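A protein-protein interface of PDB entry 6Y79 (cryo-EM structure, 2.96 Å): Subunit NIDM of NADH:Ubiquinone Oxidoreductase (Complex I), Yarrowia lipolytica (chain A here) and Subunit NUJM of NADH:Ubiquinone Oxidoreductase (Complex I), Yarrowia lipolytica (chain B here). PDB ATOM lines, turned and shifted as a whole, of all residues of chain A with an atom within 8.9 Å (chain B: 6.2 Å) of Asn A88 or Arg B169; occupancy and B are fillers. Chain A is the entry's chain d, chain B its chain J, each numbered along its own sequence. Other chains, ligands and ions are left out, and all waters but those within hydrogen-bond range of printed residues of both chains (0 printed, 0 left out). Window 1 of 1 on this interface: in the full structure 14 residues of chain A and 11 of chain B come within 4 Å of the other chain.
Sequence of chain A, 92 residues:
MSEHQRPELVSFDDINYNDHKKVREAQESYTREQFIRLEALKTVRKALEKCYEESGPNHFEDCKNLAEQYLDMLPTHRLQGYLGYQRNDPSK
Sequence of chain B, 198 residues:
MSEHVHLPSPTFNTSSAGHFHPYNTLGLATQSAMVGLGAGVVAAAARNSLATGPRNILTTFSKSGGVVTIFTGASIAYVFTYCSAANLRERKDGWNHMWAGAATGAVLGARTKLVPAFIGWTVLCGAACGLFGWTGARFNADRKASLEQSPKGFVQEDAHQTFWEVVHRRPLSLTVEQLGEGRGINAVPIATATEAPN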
ATOM      1  N   SER A  11       5.038  -4.670   3.665  1.00  0.00           N
ATOM      2  CA  SER A  11       5.979  -3.789   4.320  1.00  0.00           C
ATOM      3  C   SER A  11       5.786  -3.826   5.833  1.00  0.00           C
ATOM      4  O   SER A  11       4.820  -4.389   6.353  1.00  0.00           O
ATOM      5  CB  SER A  11       5.842  -2.368   3.794  1.00  0.00           C
ATOM      6  OG  SER A  11       6.580  -1.485   4.605  1.00  0.00           O
ATOM      7  N   PHE A  12       6.732  -3.206   6.544  1.00  0.00           N
ATOM      8  CA  PHE A  12       6.670  -3.111   7.997  1.00  0.00           C
ATOM      9  C   PHE A  12       5.813  -1.958   8.476  1.00  0.00           C
ATOM     10  O   PHE A  12       5.601  -1.829   9.682  1.00  0.00           O
ATOM     11  CB  PHE A  12       8.062  -2.917   8.606  1.00  0.00           C
ATOM     12  CG  PHE A  12       8.966  -4.094   8.467  1.00  0.00           C
ATOM     13  CD1 PHE A  12       8.819  -5.204   9.281  1.00  0.00           C
ATOM     14  CD2 PHE A  12       9.982  -4.082   7.532  1.00  0.00           C
ATOM     15  CE1 PHE A  12       9.661  -6.286   9.146  1.00  0.00           C
ATOM     16  CE2 PHE A  12      10.823  -5.156   7.397  1.00  0.00           C
ATOM     17  CZ  PHE A  12      10.663  -6.259   8.204  1.00  0.00           C
ATOM     18  N   ASP A  13       5.321  -1.118   7.573  1.00  0.00           N
ATOM     19  CA  ASP A  13       4.802   0.192   7.929  1.00  0.00           C
ATOM     20  C   ASP A  13       3.288   0.289   7.835  1.00  0.00           C
ATOM     21  O   ASP A  13       2.670   0.978   8.652  1.00  0.00           O
ATOM     22  CB  ASP A  13       5.458   1.236   7.036  1.00  0.00           C
ATOM     23  CG  ASP A  13       6.957   1.109   7.030  1.00  0.00           C
ATOM     24  OD1 ASP A  13       7.544   1.034   8.129  1.00  0.00           O
ATOM     25  OD2 ASP A  13       7.553   1.070   5.938  1.00  0.00           O
ATOM     26  N   ASP A  14       2.678  -0.385   6.861  1.00  0.00           N
ATOM     27  CA  ASP A  14       1.227  -0.474   6.808  1.00  0.00           C
ATOM     28  C   ASP A  14       0.650  -1.392   7.873  1.00  0.00           C
ATOM     29  O   ASP A  14      -0.511  -1.215   8.260  1.00  0.00           O
ATOM     30  CB  ASP A  14       0.782  -0.969   5.435  1.00  0.00           C
ATOM     31  CG  ASP A  14       1.514  -2.238   5.003  1.00  0.00           C
ATOM     32  OD1 ASP A  14       2.511  -2.606   5.645  1.00  0.00           O
ATOM     33  OD2 ASP A  14       1.029  -2.885   4.052  1.00  0.00           O
ATOM     34  N   ILE A  15       1.438  -2.324   8.390  1.00  0.00           N
ATOM     35  CA  ILE A  15       0.890  -3.413   9.183  1.00  0.00           C
ATOM     36  C   ILE A  15       0.794  -3.029  10.647  1.00  0.00           C
ATOM     37  O   ILE A  15       1.533  -2.178  11.154  1.00  0.00           O
ATOM     38  CB  ILE A  15       1.735  -4.685   9.004  1.00  0.00           C
ATOM     39  CG1 ILE A  15       3.188  -4.430   9.406  1.00  0.00           C
ATOM     40  CG2 ILE A  15       1.663  -5.150   7.575  1.00  0.00           C
ATOM     41  CD1 ILE A  15       4.011  -5.677   9.478  1.00  0.00           C
ATOM     42  N   TYR A  17       1.595  -4.529  14.255  1.00  0.00           N
ATOM     43  CA  TYR A  17       2.530  -5.518  14.766  1.00  0.00           C
ATOM     44  C   TYR A  17       1.880  -6.497  15.731  1.00  0.00           C
ATOM     45  O   TYR A  17       2.521  -7.475  16.123  1.00  0.00           O
ATOM     46  CB  TYR A  17       3.722  -4.842  15.442  1.00  0.00           C
ATOM     47  CG  TYR A  17       4.702  -4.204  14.483  1.00  0.00           C
ATOM     48  CD1 TYR A  17       4.646  -4.456  13.119  1.00  0.00           C
ATOM     49  CD2 TYR A  17       5.691  -3.359  14.945  1.00  0.00           C
ATOM     50  CE1 TYR A  17       5.540  -3.872  12.252  1.00  0.00           C
ATOM     51  CE2 TYR A  17       6.586  -2.776  14.087  1.00  0.00           C
ATOM     52  CZ  TYR A  17       6.507  -3.035  12.747  1.00  0.00           C
ATOM     53  OH  TYR A  17       7.407  -2.443  11.901  1.00  0.00           O
ATOM     54  N   ALA A  26       6.172  -9.592   6.227  1.00  0.00           N
ATOM     55  CA  ALA A  26       6.995  -8.420   5.936  1.00  0.00           C
ATOM     56  C   ALA A  26       8.464  -8.722   6.170  1.00  0.00           C
ATOM     57  O   ALA A  26       9.338  -8.271   5.414  1.00  0.00           O
ATOM     58  CB  ALA A  26       6.552  -7.245   6.801  1.00  0.00           C
ATOM     59  N   TYR A  30      11.187  -8.552   3.063  1.00  0.00           N
ATOM     60  CA  TYR A  30      12.408  -7.756   3.109  1.00  0.00           C
ATOM     61  C   TYR A  30      13.652  -8.630   2.937  1.00  0.00           C
ATOM     62  O   TYR A  30      14.599  -8.256   2.221  1.00  0.00           O
ATOM     63  CB  TYR A  30      12.408  -7.005   4.439  1.00  0.00           C
ATOM     64  CG  TYR A  30      13.427  -5.931   4.645  1.00  0.00           C
ATOM     65  CD1 TYR A  30      13.194  -4.630   4.240  1.00  0.00           C
ATOM     66  CD2 TYR A  30      14.594  -6.207   5.314  1.00  0.00           C
ATOM     67  CE1 TYR A  30      14.127  -3.644   4.466  1.00  0.00           C
ATOM     68  CE2 TYR A  30      15.523  -5.237   5.549  1.00  0.00           C
ATOM     69  CZ  TYR A  30      15.292  -3.958   5.123  1.00  0.00           C
ATOM     70  OH  TYR A  30      16.240  -2.996   5.363  1.00  0.00           O
ATOM     71  N   TYR A  82      16.395  -7.610   8.594  1.00  0.00           N
ATOM     72  CA  TYR A  82      15.136  -6.904   8.780  1.00  0.00           C
ATOM     73  C   TYR A  82      15.060  -6.179  10.110  1.00  0.00           C
ATOM     74  O   TYR A  82      14.225  -5.279  10.250  1.00  0.00           O
ATOM     75  CB  TYR A  82      13.961  -7.877   8.658  1.00  0.00           C
ATOM     76  CG  TYR A  82      13.965  -9.015   9.655  1.00  0.00           C
ATOM     77  CD1 TYR A  82      13.384  -8.876  10.911  1.00  0.00           C
ATOM     78  CD2 TYR A  82      14.522 -10.239   9.328  1.00  0.00           C
ATOM     79  CE1 TYR A  82      13.394  -9.895  11.811  1.00  0.00           C
ATOM     80  CE2 TYR A  82      14.520 -11.272  10.227  1.00  0.00           C
ATOM     81  CZ  TYR A  82      13.959 -11.089  11.467  1.00  0.00           C
ATOM     82  OH  TYR A  82      13.941 -12.113  12.379  1.00  0.00           O
ATOM     83  N   LEU A  83      15.875  -6.597  11.085  1.00  0.00           N
ATOM     84  CA  LEU A  83      15.787  -6.076  12.446  1.00  0.00           C
ATOM     85  C   LEU A  83      16.074  -4.594  12.492  1.00  0.00           C
ATOM     86  O   LEU A  83      15.390  -3.851  13.190  1.00  0.00           O
ATOM     87  CB  LEU A  83      16.761  -6.804  13.367  1.00  0.00           C
ATOM     88  CG  LEU A  83      16.468  -8.221  13.840  1.00  0.00           C
ATOM     89  CD1 LEU A  83      17.610  -8.684  14.699  1.00  0.00           C
ATOM     90  CD2 LEU A  83      15.177  -8.261  14.618  1.00  0.00           C
ATOM     91  N   GLY A  84      17.061  -4.138  11.731  1.00  0.00           N
ATOM     92  CA  GLY A  84      17.437  -2.741  11.802  1.00  0.00           C
ATOM     93  C   GLY A  84      16.384  -1.795  11.266  1.00  0.00           C
ATOM     94  O   GLY A  84      16.284  -0.656  11.726  1.00  0.00           O
ATOM     95  N   TYR A  85      15.570  -2.249  10.318  1.00  0.00           N
ATOM     96  CA  TYR A  85      14.475  -1.416   9.848  1.00  0.00           C
ATOM     97  C   TYR A  85      13.199  -1.618  10.648  1.00  0.00           C
ATOM     98  O   TYR A  85      12.395  -0.689  10.752  1.00  0.00           O
ATOM     99  CB  TYR A  85      14.183  -1.673   8.367  1.00  0.00           C
ATOM    100  CG  TYR A  85      13.193  -0.687   7.790  1.00  0.00           C
ATOM    101  CD1 TYR A  85      13.552   0.636   7.571  1.00  0.00           C
ATOM    102  CD2 TYR A  85      11.894  -1.069   7.496  1.00  0.00           C
ATOM    103  CE1 TYR A  85      12.651   1.542   7.062  1.00  0.00           C
ATOM    104  CE2 TYR A  85      10.987  -0.170   6.988  1.00  0.00           C
ATOM    105  CZ  TYR A  85      11.373   1.135   6.776  1.00  0.00           C
ATOM    106  OH  TYR A  85      10.470   2.034   6.270  1.00  0.00           O
ATOM    107  N   GLN A  86      12.972  -2.798  11.219  1.00  0.00           N
ATOM    108  CA  GLN A  86      11.727  -2.990  11.944  1.00  0.00           C
ATOM    109  C   GLN A  86      11.791  -2.532  13.396  1.00  0.00           C
ATOM    110  O   GLN A  86      10.741  -2.314  14.000  1.00  0.00           O
ATOM    111  CB  GLN A  86      11.291  -4.451  11.885  1.00  0.00           C
ATOM    112  CG  GLN A  86      11.866  -5.317  12.958  1.00  0.00           C
ATOM    113  CD  GLN A  86      11.170  -6.639  13.051  1.00  0.00           C
ATOM    114  OE1 GLN A  86      10.267  -6.926  12.279  1.00  0.00           O
ATOM    115  NE2 GLN A  86      11.588  -7.462  13.992  1.00  0.00           N
ATOM    116  N   ARG A  87      12.981  -2.371  13.971  1.00  0.00           N
ATOM    117  CA  ARG A  87      13.068  -1.860  15.330  1.00  0.00           C
ATOM    118  C   ARG A  87      13.088  -0.346  15.369  1.00  0.00           C
ATOM    119  O   ARG A  87      12.803   0.232  16.417  1.00  0.00           O
ATOM    120  CB  ARG A  87      14.326  -2.374  16.040  1.00  0.00           C
ATOM    121  CG  ARG A  87      14.460  -3.879  16.184  1.00  0.00           C
ATOM    122  CD  ARG A  87      13.692  -4.420  17.313  1.00  0.00           C
ATOM    123  NE  ARG A  87      14.180  -3.878  18.566  1.00  0.00           N
ATOM    124  CZ  ARG A  87      14.968  -4.525  19.407  1.00  0.00           C
ATOM    125  NH1 ARG A  87      15.357  -5.750  19.131  1.00  0.00           N
ATOM    126  NH2 ARG A  87      15.358  -3.942  20.528  1.00  0.00           N
ATOM    127  N   ASN A  88      13.428   0.305  14.265  1.00  0.00           N
ATOM    128  CA  ASN A  88      13.630   1.743  14.232  1.00  0.00           C
ATOM    129  C   ASN A  88      12.828   2.350  13.098  1.00  0.00           C
ATOM    130  O   ASN A  88      12.808   1.809  11.994  1.00  0.00           O
ATOM    131  CB  ASN A  88      15.098   2.087  14.045  1.00  0.00           C
ATOM    132  CG  ASN A  88      15.951   1.553  15.147  1.00  0.00           C
ATOM    133  OD1 ASN A  88      15.690   1.802  16.318  1.00  0.00           O
ATOM    134  ND2 ASN A  88      16.971   0.795  14.791  1.00  0.00           N
ATOM    135  N   ASP A  89      12.179   3.483  13.349  1.00  0.00           N
ATOM    136  CA  ASP A  89      11.594   4.208  12.233  1.00  0.00           C
ATOM    137  C   ASP A  89      12.404   5.456  11.926  1.00  0.00           C
ATOM    138  O   ASP A  89      12.625   6.293  12.816  1.00  0.00           O
ATOM    139  CB  ASP A  89      10.111   4.565  12.436  1.00  0.00           C
ATOM    140  CG  ASP A  89       9.782   5.134  13.806  1.00  0.00           C
ATOM    141  OD1 ASP A  89      10.678   5.474  14.587  1.00  0.00           O
ATOM    142  OD2 ASP A  89       8.576   5.237  14.112  1.00  0.00           O
ATOM    143  N   PRO A  90      12.854   5.626  10.691  1.00  0.00           N
ATOM    144  CA  PRO A  90      13.280   6.952  10.260  1.00  0.00           C
ATOM    145  C   PRO A  90      12.061   7.849  10.127  1.00  0.00           C
ATOM    146  O   PRO A  90      10.914   7.397  10.149  1.00  0.00           O
ATOM    147  CB  PRO A  90      13.932   6.705   8.900  1.00  0.00           C
ATOM    148  CG  PRO A  90      13.394   5.388   8.438  1.00  0.00           C
ATOM    149  CD  PRO A  90      12.765   4.668   9.579  1.00  0.00           C
ATOM    150  N   SER A  91      12.334   9.145  10.024  1.00  0.00           N
ATOM    151  CA  SER A  91      11.339  10.228   9.964  1.00  0.00           C
ATOM    152  C   SER A  91      10.416  10.217  11.190  1.00  0.00           C
ATOM    153  O   SER A  91       9.196  10.412  11.092  1.00  0.00           O
ATOM    154  CB  SER A  91      10.529  10.216   8.663  1.00  0.00           C
ATOM    155  OG  SER A  91       9.559   9.154   8.697  1.00  0.00           O
ATOM    156  N   LYS A  92      11.019  10.002  12.367  1.00  0.00           N
ATOM    157  CA  LYS A  92      10.279  10.000  13.612  1.00  0.00           C
ATOM    158  C   LYS A  92      11.139  10.346  14.839  1.00  0.00           C
ATOM    159  O   LYS A  92      12.369  10.475  14.759  1.00  0.00           O
ATOM    160  CB  LYS A  92       9.628   8.643  13.824  1.00  0.00           C
ATOM    161  CG  LYS A  92       8.686   8.590  15.005  1.00  0.00           C
ATOM    162  CD  LYS A  92       7.483   9.477  14.752  1.00  0.00           C
ATOM    163  CE  LYS A  92       6.517   9.436  15.920  1.00  0.00           C
ATOM    164  NZ  LYS A  92       5.869   8.106  16.048  1.00  0.00           N
ATOM    165  N   ASP B 158       2.349   7.488  21.295  1.00  0.00           N
ATOM    166  CA  ASP B 158       3.774   7.722  21.107  1.00  0.00           C
ATOM    167  C   ASP B 158       4.267   8.844  22.008  1.00  0.00           C
ATOM    168  O   ASP B 158       3.714   9.949  22.018  1.00  0.00           O
ATOM    169  CB  ASP B 158       4.063   8.040  19.643  1.00  0.00           C
ATOM    170  CG  ASP B 158       3.881   6.830  18.744  1.00  0.00           C
ATOM    171  OD1 ASP B 158       4.075   5.697  19.227  1.00  0.00           O
ATOM    172  OD2 ASP B 158       3.546   7.013  17.555  1.00  0.00           O
ATOM    173  N   GLN B 161       9.761   7.033  25.546  1.00  0.00           N
ATOM    174  CA  GLN B 161       9.710   5.727  26.194  1.00  0.00           C
ATOM    175  C   GLN B 161      10.539   5.765  27.467  1.00  0.00           C
ATOM    176  O   GLN B 161      11.745   6.020  27.428  1.00  0.00           O
ATOM    177  CB  GLN B 161      10.217   4.640  25.251  1.00  0.00           C
ATOM    178  CG  GLN B 161      10.545   3.338  25.950  1.00  0.00           C
ATOM    179  CD  GLN B 161      11.096   2.294  25.022  1.00  0.00           C
ATOM    180  OE1 GLN B 161      11.344   2.557  23.850  1.00  0.00           O
ATOM    181  NE2 GLN B 161      11.278   1.090  25.535  1.00  0.00           N
ATOM    182  N   VAL B 167       8.134  -0.549  23.599  1.00  0.00           N
ATOM    183  CA  VAL B 167       7.470  -0.106  22.388  1.00  0.00           C
ATOM    184  C   VAL B 167       7.617  -1.193  21.330  1.00  0.00           C
ATOM    185  O   VAL B 167       8.219  -2.234  21.565  1.00  0.00           O
ATOM    186  CB  VAL B 167       8.022   1.234  21.869  1.00  0.00           C
ATOM    187  CG1 VAL B 167       7.861   2.313  22.905  1.00  0.00           C
ATOM    188  CG2 VAL B 167       9.462   1.090  21.498  1.00  0.00           C
ATOM    189  N   HIS B 168       7.033  -0.943  20.162  1.00  0.00           N
ATOM    190  CA  HIS B 168       7.218  -1.796  18.998  1.00  0.00           C
ATOM    191  C   HIS B 168       8.349  -1.288  18.115  1.00  0.00           C
ATOM    192  O   HIS B 168       9.170  -2.072  17.637  1.00  0.00           O
ATOM    193  CB  HIS B 168       5.930  -1.872  18.180  1.00  0.00           C
ATOM    194  CG  HIS B 168       4.851  -2.695  18.804  1.00  0.00           C
ATOM    195  ND1 HIS B 168       3.819  -2.140  19.527  1.00  0.00           N
ATOM    196  CD2 HIS B 168       4.631  -4.030  18.799  1.00  0.00           C
ATOM    197  CE1 HIS B 168       3.013  -3.099  19.946  1.00  0.00           C
ATOM    198  NE2 HIS B 168       3.485  -4.255  19.520  1.00  0.00           N
ATOM    199  N   ARG B 169       8.388   0.019  17.881  1.00  0.00           N
ATOM    200  CA  ARG B 169       9.445   0.673  17.129  1.00  0.00           C
ATOM    201  C   ARG B 169       9.967   1.851  17.926  1.00  0.00           C
ATOM    202  O   ARG B 169       9.193   2.600  18.523  1.00  0.00           O
ATOM    203  CB  ARG B 169       8.960   1.175  15.777  1.00  0.00           C
ATOM    204  CG  ARG B 169       8.611   0.098  14.793  1.00  0.00           C
ATOM    205  CD  ARG B 169       7.961   0.696  13.571  1.00  0.00           C
ATOM    206  NE  ARG B 169       8.941   1.326  12.699  1.00  0.00           N
ATOM    207  CZ  ARG B 169       9.487   0.723  11.654  1.00  0.00           C
ATOM    208  NH1 ARG B 169       9.139  -0.516  11.365  1.00  0.00           N
ATOM    209  NH2 ARG B 169      10.378   1.349  10.905  1.00  0.00           N
ATOM    210  N   ARG B 170      11.169   2.006  17.914  1.00  0.00           N
ATOM    211  CA  ARG B 170      12.060   3.000  18.468  1.00  0.00           C
ATOM    212  C   ARG B 170      12.298   4.097  17.444  1.00  0.00           C
ATOM    213  O   ARG B 170      12.209   3.844  16.248  1.00  0.00           O
ATOM    214  CB  ARG B 170      13.390   2.342  18.833  1.00  0.00           C
ATOM    215  CG  ARG B 170      14.168   3.019  19.901  1.00  0.00           C
ATOM    216  CD  ARG B 170      15.159   2.066  20.513  1.00  0.00           C
ATOM    217  NE  ARG B 170      16.280   2.788  21.080  1.00  0.00           N
ATOM    218  CZ  ARG B 170      17.367   3.067  20.388  1.00  0.00           C
ATOM    219  NH1 ARG B 170      17.449   2.670  19.133  1.00  0.00           N
ATOM    220  NH2 ARG B 170      18.360   3.734  20.939  1.00  0.00           N
ATOM    221  N   PRO B 171      12.575   5.339  17.827  1.00  0.00           N
ATOM    222  CA  PRO B 171      12.985   6.330  16.825  1.00  0.00           C
ATOM    223  C   PRO B 171      14.414   6.101  16.349  1.00  0.00           C
ATOM    224  O   PRO B 171      15.308   5.785  17.137  1.00  0.00           O
ATOM    225  CB  PRO B 171      12.852   7.665  17.569  1.00  0.00           C
ATOM    226  CG  PRO B 171      12.809   7.318  19.000  1.00  0.00           C
ATOM    227  CD  PRO B 171      12.169   5.978  19.088  1.00  0.00           C
ATOM    228  N   LEU B 172      14.622   6.268  15.035  1.00  0.00           N
ATOM    229  CA  LEU B 172      15.942   6.044  14.443  1.00  0.00           C
ATOM    230  C   LEU B 172      16.934   7.125  14.844  1.00  0.00           C
ATOM    231  O   LEU B 172      18.147   6.881  14.854  1.00  0.00           O
ATOM    232  CB  LEU B 172      15.833   5.971  12.920  1.00  0.00           C
ATOM    233  CG  LEU B 172      16.943   5.337  12.079  1.00  0.00           C
ATOM    234  CD1 LEU B 172      16.338   4.599  10.908  1.00  0.00           C
ATOM    235  CD2 LEU B 172      17.906   6.378  11.566  1.00  0.00           C
ATOM    236  N   THR B 175      18.473   5.965  17.854  1.00  0.00           N
ATOM    237  CA  THR B 175      19.452   4.934  17.535  1.00  0.00           C
ATOM    238  C   THR B 175      20.770   5.548  17.088  1.00  0.00           C
ATOM    239  O   THR B 175      21.845   5.069  17.458  1.00  0.00           O
ATOM    240  CB  THR B 175      18.896   4.015  16.450  1.00  0.00           C
ATOM    241  OG1 THR B 175      17.531   3.718  16.746  1.00  0.00           O
ATOM    242  CG2 THR B 175      19.648   2.723  16.417  1.00  0.00           C
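Of the 19 printed residues of chain A, 10 touch a printed residue of chain B.
Hydrophobic or aromatic side chains of chain A within 4 Å of the printed part of chain B: Phe A12, Tyr A17 and Pro A90.
Among the printed residues, 18 pairs touch across the chains.
NH1 of Arg B169 touches CB of Phe A12, 3.8 Å away.
His B168 touches Tyr A17.
Gln A86 touches His B168.
Arg B169 touches Gln A86 (CG to O, 3.3 Å).
Arg B169 touches Arg A87 (CA to O, 3.5 Å).
Asp A89 touches Arg B169 (CA to NH2, 3.4 Å).
Asp A89 touches Pro B171 (OD1 to CA, 3.3 Å).
Pro A90 touches Leu B172 (N to CD1, 3.6 Å).
OD2 of Asp B158 is in salt-bridge range of NZ of Lys A92, 3.0 Å away.
OD1 of Asp A13 is in salt-bridge range of NH1 of Arg B169, at 3.9 Å.
The guanidinium group of Arg B169 sits at hydrogen-bond distance from the side-chain hydroxyl of Tyr A17.
The backbone carbonyl oxygen of Tyr A85 is in hydrogen-bond range of the guanidinium group of Arg B169 (2.9 Å).
O of Asn A88 is in hydrogen-bond range of NH2 of Arg B169, 2.7 Å away.
The backbone carbonyl oxygen (O) of Arg A87 sits at hydrogen-bond distance from the backbone NH (N) of Arg B170 (2.8 Å).
The guanidinium group (NH1) of Arg B170 lies within hydrogen-bond range of the side-chain amide oxygen (OD1) of Asn A88 (3.4 Å).
The backbone carbonyl oxygen (O) of Arg B170 sits at hydrogen-bond distance from the backbone NH (N) of Asp A89, at 2.9 Å.
The backbone carbonyl oxygen (O) of Asp A89 lies within hydrogen-bond range of the backbone NH (N) of Leu B172 (3.0 Å).
OG1 of Thr B175 is in hydrogen-bond range of OD1 of Asn A88 (2.7 Å).
Printed residues of chain B within 4 Å of Tyr A17: His B168 and Arg B169.
Asn A88 touches three residues of chain B.
Of the printed residues of chain A, Asp B158 touches Lys A92 (3.0 Å).
Gln B161 touches none of the printed residues of chain A.
Arg B169 touches just these residues of chain A: Phe A12 (3.8 Å), Asp A13 (3.9 Å), Tyr A17 (2.6 Å), Tyr A85 (2.9 Å), Gln A86 (3.3 Å), Arg A87 (3.5 Å), Asn A88 (2.7 Å) and Asp A89 (3.4 Å).
The guanidinium group of Arg B170 lies within hydrogen-bond range of the side-chain hydroxyl of Thr B175 (2.6 Å).
The backbone carbonyl oxygen of Pro B171 lies within hydrogen-bond range of the side-chain hydroxyl of Thr B175, at 3.1 Å.
The side-chain hydroxyl (OG) of Ser A11 lies within hydrogen-bond range of the side-chain carboxylate (OD2) of Asp A13, 3.0 Å away.
The backbone carbonyl oxygen of Phe A12 sits at hydrogen-bond distance from the side-chain hydroxyl of Tyr A17 (2.9 Å).
OH of Tyr A85 lies within hydrogen-bond range of OD2 of Asp A13, at 3.1 Å.
The side-chain amide nitrogen (ND2) of Asn A88 sits at hydrogen-bond distance from the backbone carbonyl oxygen (O) of Gly A84.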
